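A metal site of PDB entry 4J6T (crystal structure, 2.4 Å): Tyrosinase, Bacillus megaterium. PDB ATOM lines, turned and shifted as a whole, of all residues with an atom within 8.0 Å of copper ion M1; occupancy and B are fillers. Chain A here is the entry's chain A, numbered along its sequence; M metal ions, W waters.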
ATOM      1  N   HIS A  42      14.562  23.398  -8.165  1.00  0.00           N
ATOM      2  CA  HIS A  42      14.187  22.002  -8.165  1.00  0.00           C
ATOM      3  C   HIS A  42      13.779  21.515  -9.558  1.00  0.00           C
ATOM      4  O   HIS A  42      14.239  20.476 -10.024  1.00  0.00           O
ATOM      5  CB  HIS A  42      13.087  21.733  -7.156  1.00  0.00           C
ATOM      6  CG  HIS A  42      12.784  20.293  -6.962  1.00  0.00           C
ATOM      7  ND1 HIS A  42      11.625  19.699  -7.407  1.00  0.00           N
ATOM      8  CD2 HIS A  42      13.521  19.300  -6.395  1.00  0.00           C
ATOM      9  CE1 HIS A  42      11.639  18.414  -7.102  1.00  0.00           C
ATOM     10  NE2 HIS A  42      12.779  18.149  -6.481  1.00  0.00           N
ATOM     11  N   GLY A  43      12.916  22.275 -10.223  1.00  0.00           N
ATOM     12  CA  GLY A  43      12.569  21.962 -11.599  1.00  0.00           C
ATOM     13  C   GLY A  43      13.804  21.947 -12.490  1.00  0.00           C
ATOM     14  O   GLY A  43      13.951  21.057 -13.339  1.00  0.00           O
ATOM     15  N   ALA A  45      16.904  21.248 -11.852  1.00  0.00           N
ATOM     16  CA  ALA A  45      17.748  20.069 -11.691  1.00  0.00           C
ATOM     17  C   ALA A  45      17.190  18.840 -12.433  1.00  0.00           C
ATOM     18  O   ALA A  45      17.959  17.993 -12.932  1.00  0.00           O
ATOM     19  CB  ALA A  45      17.925  19.771 -10.213  1.00  0.00           C
ATOM     20  N   ASN A  57      19.003  12.298 -13.303  1.00  0.00           N
ATOM     21  CA  ASN A  57      19.226  13.746 -13.312  1.00  0.00           C
ATOM     22  C   ASN A  57      19.919  14.248 -12.030  1.00  0.00           C
ATOM     23  O   ASN A  57      20.188  13.466 -11.112  1.00  0.00           O
ATOM     24  CB  ASN A  57      17.945  14.540 -13.646  1.00  0.00           C
ATOM     25  CG  ASN A  57      16.872  14.374 -12.601  1.00  0.00           C
ATOM     26  OD1 ASN A  57      16.954  14.969 -11.525  1.00  0.00           O
ATOM     27  ND2 ASN A  57      15.858  13.575 -12.915  1.00  0.00           N
ATOM     28  N   ALA A  59      19.145  15.826  -9.391  1.00  0.00           N
ATOM     29  CA  ALA A  59      18.522  15.729  -8.073  1.00  0.00           C
ATOM     30  C   ALA A  59      17.775  14.410  -7.848  1.00  0.00           C
ATOM     31  O   ALA A  59      17.459  14.080  -6.704  1.00  0.00           O
ATOM     32  CB  ALA A  59      17.592  16.903  -7.864  1.00  0.00           C
ATOM     33  N   HIS A  60      17.471  13.677  -8.911  1.00  0.00           N
ATOM     34  CA  HIS A  60      16.675  12.473  -8.773  1.00  0.00           C
ATOM     35  C   HIS A  60      17.137  11.356  -9.659  1.00  0.00           C
ATOM     36  O   HIS A  60      17.681  11.578 -10.766  1.00  0.00           O
ATOM     37  CB  HIS A  60      15.209  12.776  -9.041  1.00  0.00           C
ATOM     38  CG  HIS A  60      14.703  14.030  -8.370  1.00  0.00           C
ATOM     39  ND1 HIS A  60      14.869  15.252  -8.911  1.00  0.00           N
ATOM     40  CD2 HIS A  60      14.041  14.222  -7.157  1.00  0.00           C
ATOM     41  CE1 HIS A  60      14.332  16.176  -8.094  1.00  0.00           C
ATOM     42  NE2 HIS A  60      13.819  15.546  -7.022  1.00  0.00           N
ATOM     43  N   PHE A  65      20.696  12.184  -5.193  1.00  0.00           N
ATOM     44  CA  PHE A  65      19.362  12.457  -4.638  1.00  0.00           C
ATOM     45  C   PHE A  65      19.417  12.939  -3.200  1.00  0.00           C
ATOM     46  O   PHE A  65      18.857  13.995  -2.878  1.00  0.00           O
ATOM     47  CB  PHE A  65      18.484  11.218  -4.709  1.00  0.00           C
ATOM     48  CG  PHE A  65      17.202  11.325  -3.895  1.00  0.00           C
ATOM     49  CD1 PHE A  65      16.194  12.196  -4.281  1.00  0.00           C
ATOM     50  CD2 PHE A  65      17.021  10.540  -2.765  1.00  0.00           C
ATOM     51  CE1 PHE A  65      15.005  12.287  -3.558  1.00  0.00           C
ATOM     52  CE2 PHE A  65      15.835  10.619  -2.031  1.00  0.00           C
ATOM     53  CZ  PHE A  65      14.824  11.503  -2.428  1.00  0.00           C
ATOM     54  N   TRP A  68      21.855  16.344  -2.661  1.00  0.00           N
ATOM     55  CA  TRP A  68      21.202  17.478  -3.327  1.00  0.00           C
ATOM     56  C   TRP A  68      20.085  18.043  -2.447  1.00  0.00           C
ATOM     57  O   TRP A  68      20.066  19.242  -2.100  1.00  0.00           O
ATOM     58  CB  TRP A  68      20.660  17.077  -4.705  1.00  0.00           C
ATOM     59  CG  TRP A  68      20.225  18.206  -5.614  1.00  0.00           C
ATOM     60  CD1 TRP A  68      20.904  18.685  -6.705  1.00  0.00           C
ATOM     61  CD2 TRP A  68      19.012  18.978  -5.531  1.00  0.00           C
ATOM     62  NE1 TRP A  68      20.184  19.682  -7.308  1.00  0.00           N
ATOM     63  CE2 TRP A  68      19.029  19.886  -6.611  1.00  0.00           C
ATOM     64  CE3 TRP A  68      17.908  18.972  -4.669  1.00  0.00           C
ATOM     65  CZ2 TRP A  68      17.995  20.814  -6.836  1.00  0.00           C
ATOM     66  CZ3 TRP A  68      16.873  19.890  -4.896  1.00  0.00           C
ATOM     67  CH2 TRP A  68      16.930  20.792  -5.969  1.00  0.00           C
ATOM     68  N   HIS A  69      19.142  17.183  -2.070  1.00  0.00           N
ATOM     69  CA  HIS A  69      18.063  17.624  -1.209  1.00  0.00           C
ATOM     70  C   HIS A  69      18.550  18.138   0.145  1.00  0.00           C
ATOM     71  O   HIS A  69      18.003  19.105   0.674  1.00  0.00           O
ATOM     72  CB  HIS A  69      16.954  16.580  -1.120  1.00  0.00           C
ATOM     73  CG  HIS A  69      16.164  16.447  -2.392  1.00  0.00           C
ATOM     74  ND1 HIS A  69      16.607  15.703  -3.463  1.00  0.00           N
ATOM     75  CD2 HIS A  69      14.988  16.991  -2.774  1.00  0.00           C
ATOM     76  CE1 HIS A  69      15.720  15.776  -4.444  1.00  0.00           C
ATOM     77  NE2 HIS A  69      14.725  16.546  -4.049  1.00  0.00           N
ATOM     78  N   TYR A  72      19.638  21.545  -0.488  1.00  0.00           N
ATOM     79  CA  TYR A  72      18.442  22.310  -0.775  1.00  0.00           C
ATOM     80  C   TYR A  72      17.779  22.775   0.515  1.00  0.00           C
ATOM     81  O   TYR A  72      17.395  23.947   0.645  1.00  0.00           O
ATOM     82  CB  TYR A  72      17.480  21.410  -1.532  1.00  0.00           C
ATOM     83  CG  TYR A  72      16.241  22.052  -2.131  1.00  0.00           C
ATOM     84  CD1 TYR A  72      16.326  22.896  -3.243  1.00  0.00           C
ATOM     85  CD2 TYR A  72      14.979  21.732  -1.637  1.00  0.00           C
ATOM     86  CE1 TYR A  72      15.198  23.437  -3.814  1.00  0.00           C
ATOM     87  CE2 TYR A  72      13.832  22.267  -2.217  1.00  0.00           C
ATOM     88  CZ  TYR A  72      13.941  23.115  -3.306  1.00  0.00           C
ATOM     89  OH  TYR A  72      12.792  23.626  -3.868  1.00  0.00           O
ATOM     90  N   GLU A 195      14.862   6.482  -1.743  1.00  0.00           N
ATOM     91  CA  GLU A 195      14.213   7.234  -2.798  1.00  0.00           C
ATOM     92  C   GLU A 195      12.932   6.505  -3.205  1.00  0.00           C
ATOM     93  O   GLU A 195      11.900   7.124  -3.478  1.00  0.00           O
ATOM     94  CB  GLU A 195      15.141   7.455  -3.992  1.00  0.00           C
ATOM     95  CG  GLU A 195      14.604   8.514  -4.957  1.00  0.00           C
ATOM     96  CD  GLU A 195      15.537   8.845  -6.136  1.00  0.00           C
ATOM     97  OE1 GLU A 195      15.229   9.806  -6.884  1.00  0.00           O
ATOM     98  OE2 GLU A 195      16.559   8.148  -6.333  1.00  0.00           O
ATOM     99  N   HIS A 204      10.116   7.552  -0.117  1.00  0.00           N
ATOM    100  CA  HIS A 204      10.061   8.899  -0.678  1.00  0.00           C
ATOM    101  C   HIS A 204       9.069   9.067  -1.830  1.00  0.00           C
ATOM    102  O   HIS A 204       8.180   9.914  -1.764  1.00  0.00           O
ATOM    103  CB  HIS A 204      11.445   9.360  -1.132  1.00  0.00           C
ATOM    104  CG  HIS A 204      11.427  10.575  -2.014  1.00  0.00           C
ATOM    105  ND1 HIS A 204      11.583  10.514  -3.380  1.00  0.00           N
ATOM    106  CD2 HIS A 204      11.252  11.884  -1.715  1.00  0.00           C
ATOM    107  CE1 HIS A 204      11.520  11.729  -3.884  1.00  0.00           C
ATOM    108  NE2 HIS A 204      11.322  12.587  -2.884  1.00  0.00           N
ATOM    109  N   ASN A 205       9.226   8.264  -2.887  1.00  0.00           N
ATOM    110  CA  ASN A 205       8.301   8.336  -4.008  1.00  0.00           C
ATOM    111  C   ASN A 205       6.849   8.154  -3.574  1.00  0.00           C
ATOM    112  O   ASN A 205       5.942   8.795  -4.119  1.00  0.00           O
ATOM    113  CB  ASN A 205       8.641   7.300  -5.085  1.00  0.00           C
ATOM    114  CG  ASN A 205       9.927   7.621  -5.834  1.00  0.00           C
ATOM    115  OD1 ASN A 205      10.367   8.779  -5.866  1.00  0.00           O
ATOM    116  ND2 ASN A 205      10.540   6.602  -6.461  1.00  0.00           N
ATOM    117  N   HIS A 208       5.184  11.345  -1.998  1.00  0.00           N
ATOM    118  CA  HIS A 208       4.791  12.216  -3.097  1.00  0.00           C
ATOM    119  C   HIS A 208       3.458  11.804  -3.745  1.00  0.00           C
ATOM    120  O   HIS A 208       2.581  12.649  -3.962  1.00  0.00           O
ATOM    121  CB  HIS A 208       5.900  12.238  -4.164  1.00  0.00           C
ATOM    122  CG  HIS A 208       7.041  13.138  -3.813  1.00  0.00           C
ATOM    123  ND1 HIS A 208       7.007  14.504  -3.984  1.00  0.00           N
ATOM    124  CD2 HIS A 208       8.269  12.860  -3.297  1.00  0.00           C
ATOM    125  CE1 HIS A 208       8.151  15.026  -3.588  1.00  0.00           C
ATOM    126  NE2 HIS A 208       8.937  14.054  -3.173  1.00  0.00           N
ATOM    127  N   VAL A 218       6.697  15.627  -9.619  1.00  0.00           N
ATOM    128  CA  VAL A 218       8.005  16.094  -9.142  1.00  0.00           C
ATOM    129  C   VAL A 218       8.358  17.575  -9.431  1.00  0.00           C
ATOM    130  O   VAL A 218       8.755  18.283  -8.516  1.00  0.00           O
ATOM    131  CB  VAL A 218       9.180  15.190  -9.603  1.00  0.00           C
ATOM    132  CG1 VAL A 218      10.477  15.570  -8.864  1.00  0.00           C
ATOM    133  CG2 VAL A 218       8.821  13.723  -9.394  1.00  0.00           C
ATOM    134  N   PRO A 219       8.184  18.038 -10.687  1.00  0.00           N
ATOM    135  CA  PRO A 219       8.608  19.425 -10.954  1.00  0.00           C
ATOM    136  C   PRO A 219       7.731  20.523 -10.297  1.00  0.00           C
ATOM    137  O   PRO A 219       8.149  21.672 -10.207  1.00  0.00           O
ATOM    138  CB  PRO A 219       8.528  19.537 -12.487  1.00  0.00           C
ATOM    139  CG  PRO A 219       8.530  18.100 -12.982  1.00  0.00           C
ATOM    140  CD  PRO A 219       7.819  17.325 -11.931  1.00  0.00           C
ATOM    141  N   ALA A 221       6.339  19.896  -7.204  1.00  0.00           N
ATOM    142  CA  ALA A 221       6.267  19.497  -5.788  1.00  0.00           C
ATOM    143  C   ALA A 221       6.589  20.573  -4.708  1.00  0.00           C
ATOM    144  O   ALA A 221       5.849  20.694  -3.729  1.00  0.00           O
ATOM    145  CB  ALA A 221       7.070  18.208  -5.559  1.00  0.00           C
ATOM    146  N   PRO A 222       7.673  21.359  -4.885  1.00  0.00           N
ATOM    147  CA  PRO A 222       7.956  22.389  -3.862  1.00  0.00           C
ATOM    148  C   PRO A 222       6.888  23.470  -3.663  1.00  0.00           C
ATOM    149  O   PRO A 222       6.948  24.183  -2.660  1.00  0.00           O
ATOM    150  CB  PRO A 222       9.284  23.005  -4.345  1.00  0.00           C
ATOM    151  CG  PRO A 222       9.951  21.850  -5.107  1.00  0.00           C
ATOM    152  CD  PRO A 222       8.818  21.166  -5.806  1.00  0.00           C
ATOM    153  N   PHE A 227       6.457  19.834   1.200  1.00  0.00           N
ATOM    154  CA  PHE A 227       7.600  19.270   0.465  1.00  0.00           C
ATOM    155  C   PHE A 227       8.887  19.285   1.311  1.00  0.00           C
ATOM    156  O   PHE A 227       9.648  18.320   1.304  1.00  0.00           O
ATOM    157  CB  PHE A 227       7.828  20.042  -0.855  1.00  0.00           C
ATOM    158  CG  PHE A 227       9.060  19.607  -1.632  1.00  0.00           C
ATOM    159  CD1 PHE A 227      10.290  20.199  -1.398  1.00  0.00           C
ATOM    160  CD2 PHE A 227       8.976  18.579  -2.573  1.00  0.00           C
ATOM    161  CE1 PHE A 227      11.421  19.782  -2.088  1.00  0.00           C
ATOM    162  CE2 PHE A 227      10.101  18.165  -3.276  1.00  0.00           C
ATOM    163  CZ  PHE A 227      11.328  18.766  -3.031  1.00  0.00           C
ATOM    164  N   HIS A 230       8.517  17.066   4.398  1.00  0.00           N
ATOM    165  CA  HIS A 230       8.719  15.693   3.982  1.00  0.00           C
ATOM    166  C   HIS A 230      10.205  15.385   3.749  1.00  0.00           C
ATOM    167  O   HIS A 230      10.711  14.333   4.179  1.00  0.00           O
ATOM    168  CB  HIS A 230       7.965  15.402   2.708  1.00  0.00           C
ATOM    169  CG  HIS A 230       8.507  14.219   1.962  1.00  0.00           C
ATOM    170  ND1 HIS A 230       9.043  14.319   0.692  1.00  0.00           N
ATOM    171  CD2 HIS A 230       8.656  12.935   2.342  1.00  0.00           C
ATOM    172  CE1 HIS A 230       9.448  13.120   0.303  1.00  0.00           C
ATOM    173  NE2 HIS A 230       9.229  12.264   1.284  1.00  0.00           N
ATOM    174  N   HIS A 231      10.878  16.306   3.053  1.00  0.00           N
ATOM    175  CA  HIS A 231      12.276  16.071   2.699  1.00  0.00           C
ATOM    176  C   HIS A 231      13.184  16.127   3.917  1.00  0.00           C
ATOM    177  O   HIS A 231      14.193  15.436   3.981  1.00  0.00           O
ATOM    178  CB  HIS A 231      12.739  16.993   1.573  1.00  0.00           C
ATOM    179  CG  HIS A 231      12.622  16.358   0.231  1.00  0.00           C
ATOM    180  ND1 HIS A 231      13.548  15.458  -0.245  1.00  0.00           N
ATOM    181  CD2 HIS A 231      11.638  16.435  -0.705  1.00  0.00           C
ATOM    182  CE1 HIS A 231      13.155  15.013  -1.426  1.00  0.00           C
ATOM    183  NE2 HIS A 231      12.009  15.601  -1.733  1.00  0.00           N
HETATM  184 CU    CU M   1      12.896  16.296  -5.364  1.00  0.00          CU
HETATM  185 CU    CU M   2      11.027  14.700  -3.554  1.00  0.00          CU
HETATM  186  O   HOH W   1      10.387  15.401  -5.586  1.00  0.00           O
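Copper ion M1 is bound by a ring nitrogen (NE2) of His 60 (2.0 Å), a ring nitrogen (NE2) of His 42 (2.2 Å) and a ring nitrogen (NE2) of His 69 (2.3 Å). Copper ion M1 has three donor atoms within binding distance. Slightly farther from copper ion M1 lies water W1 (2.7 Å).
A ring nitrogen (ND1) of His 42 sits close to the backbone carbonyl oxygen of Val 218, 3.4 Å away. The backbone NH (N) of His 60 sits at hydrogen-bond distance from the side-chain amide oxygen (OD1) of Asn 57, at 3.0 Å. A ring nitrogen (ND1) of His 69 is in hydrogen-bond range of the backbone carbonyl oxygen of Phe 65 (2.9 Å).
CZ of Phe 227 touches copper ion M1, at 3.7 Å. NE2 of His 231 touches copper ion M1, at 3.8 Å. Within 4 Å of copper ion M1: His 42, His 60, His 69, Phe 227 and His 231. Along chain A the residues within 4 Å of copper ion M1 span positions 42 to 231. The nearest printed residue that does not touch copper ion M1 is Val 218 (4.3 Å).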
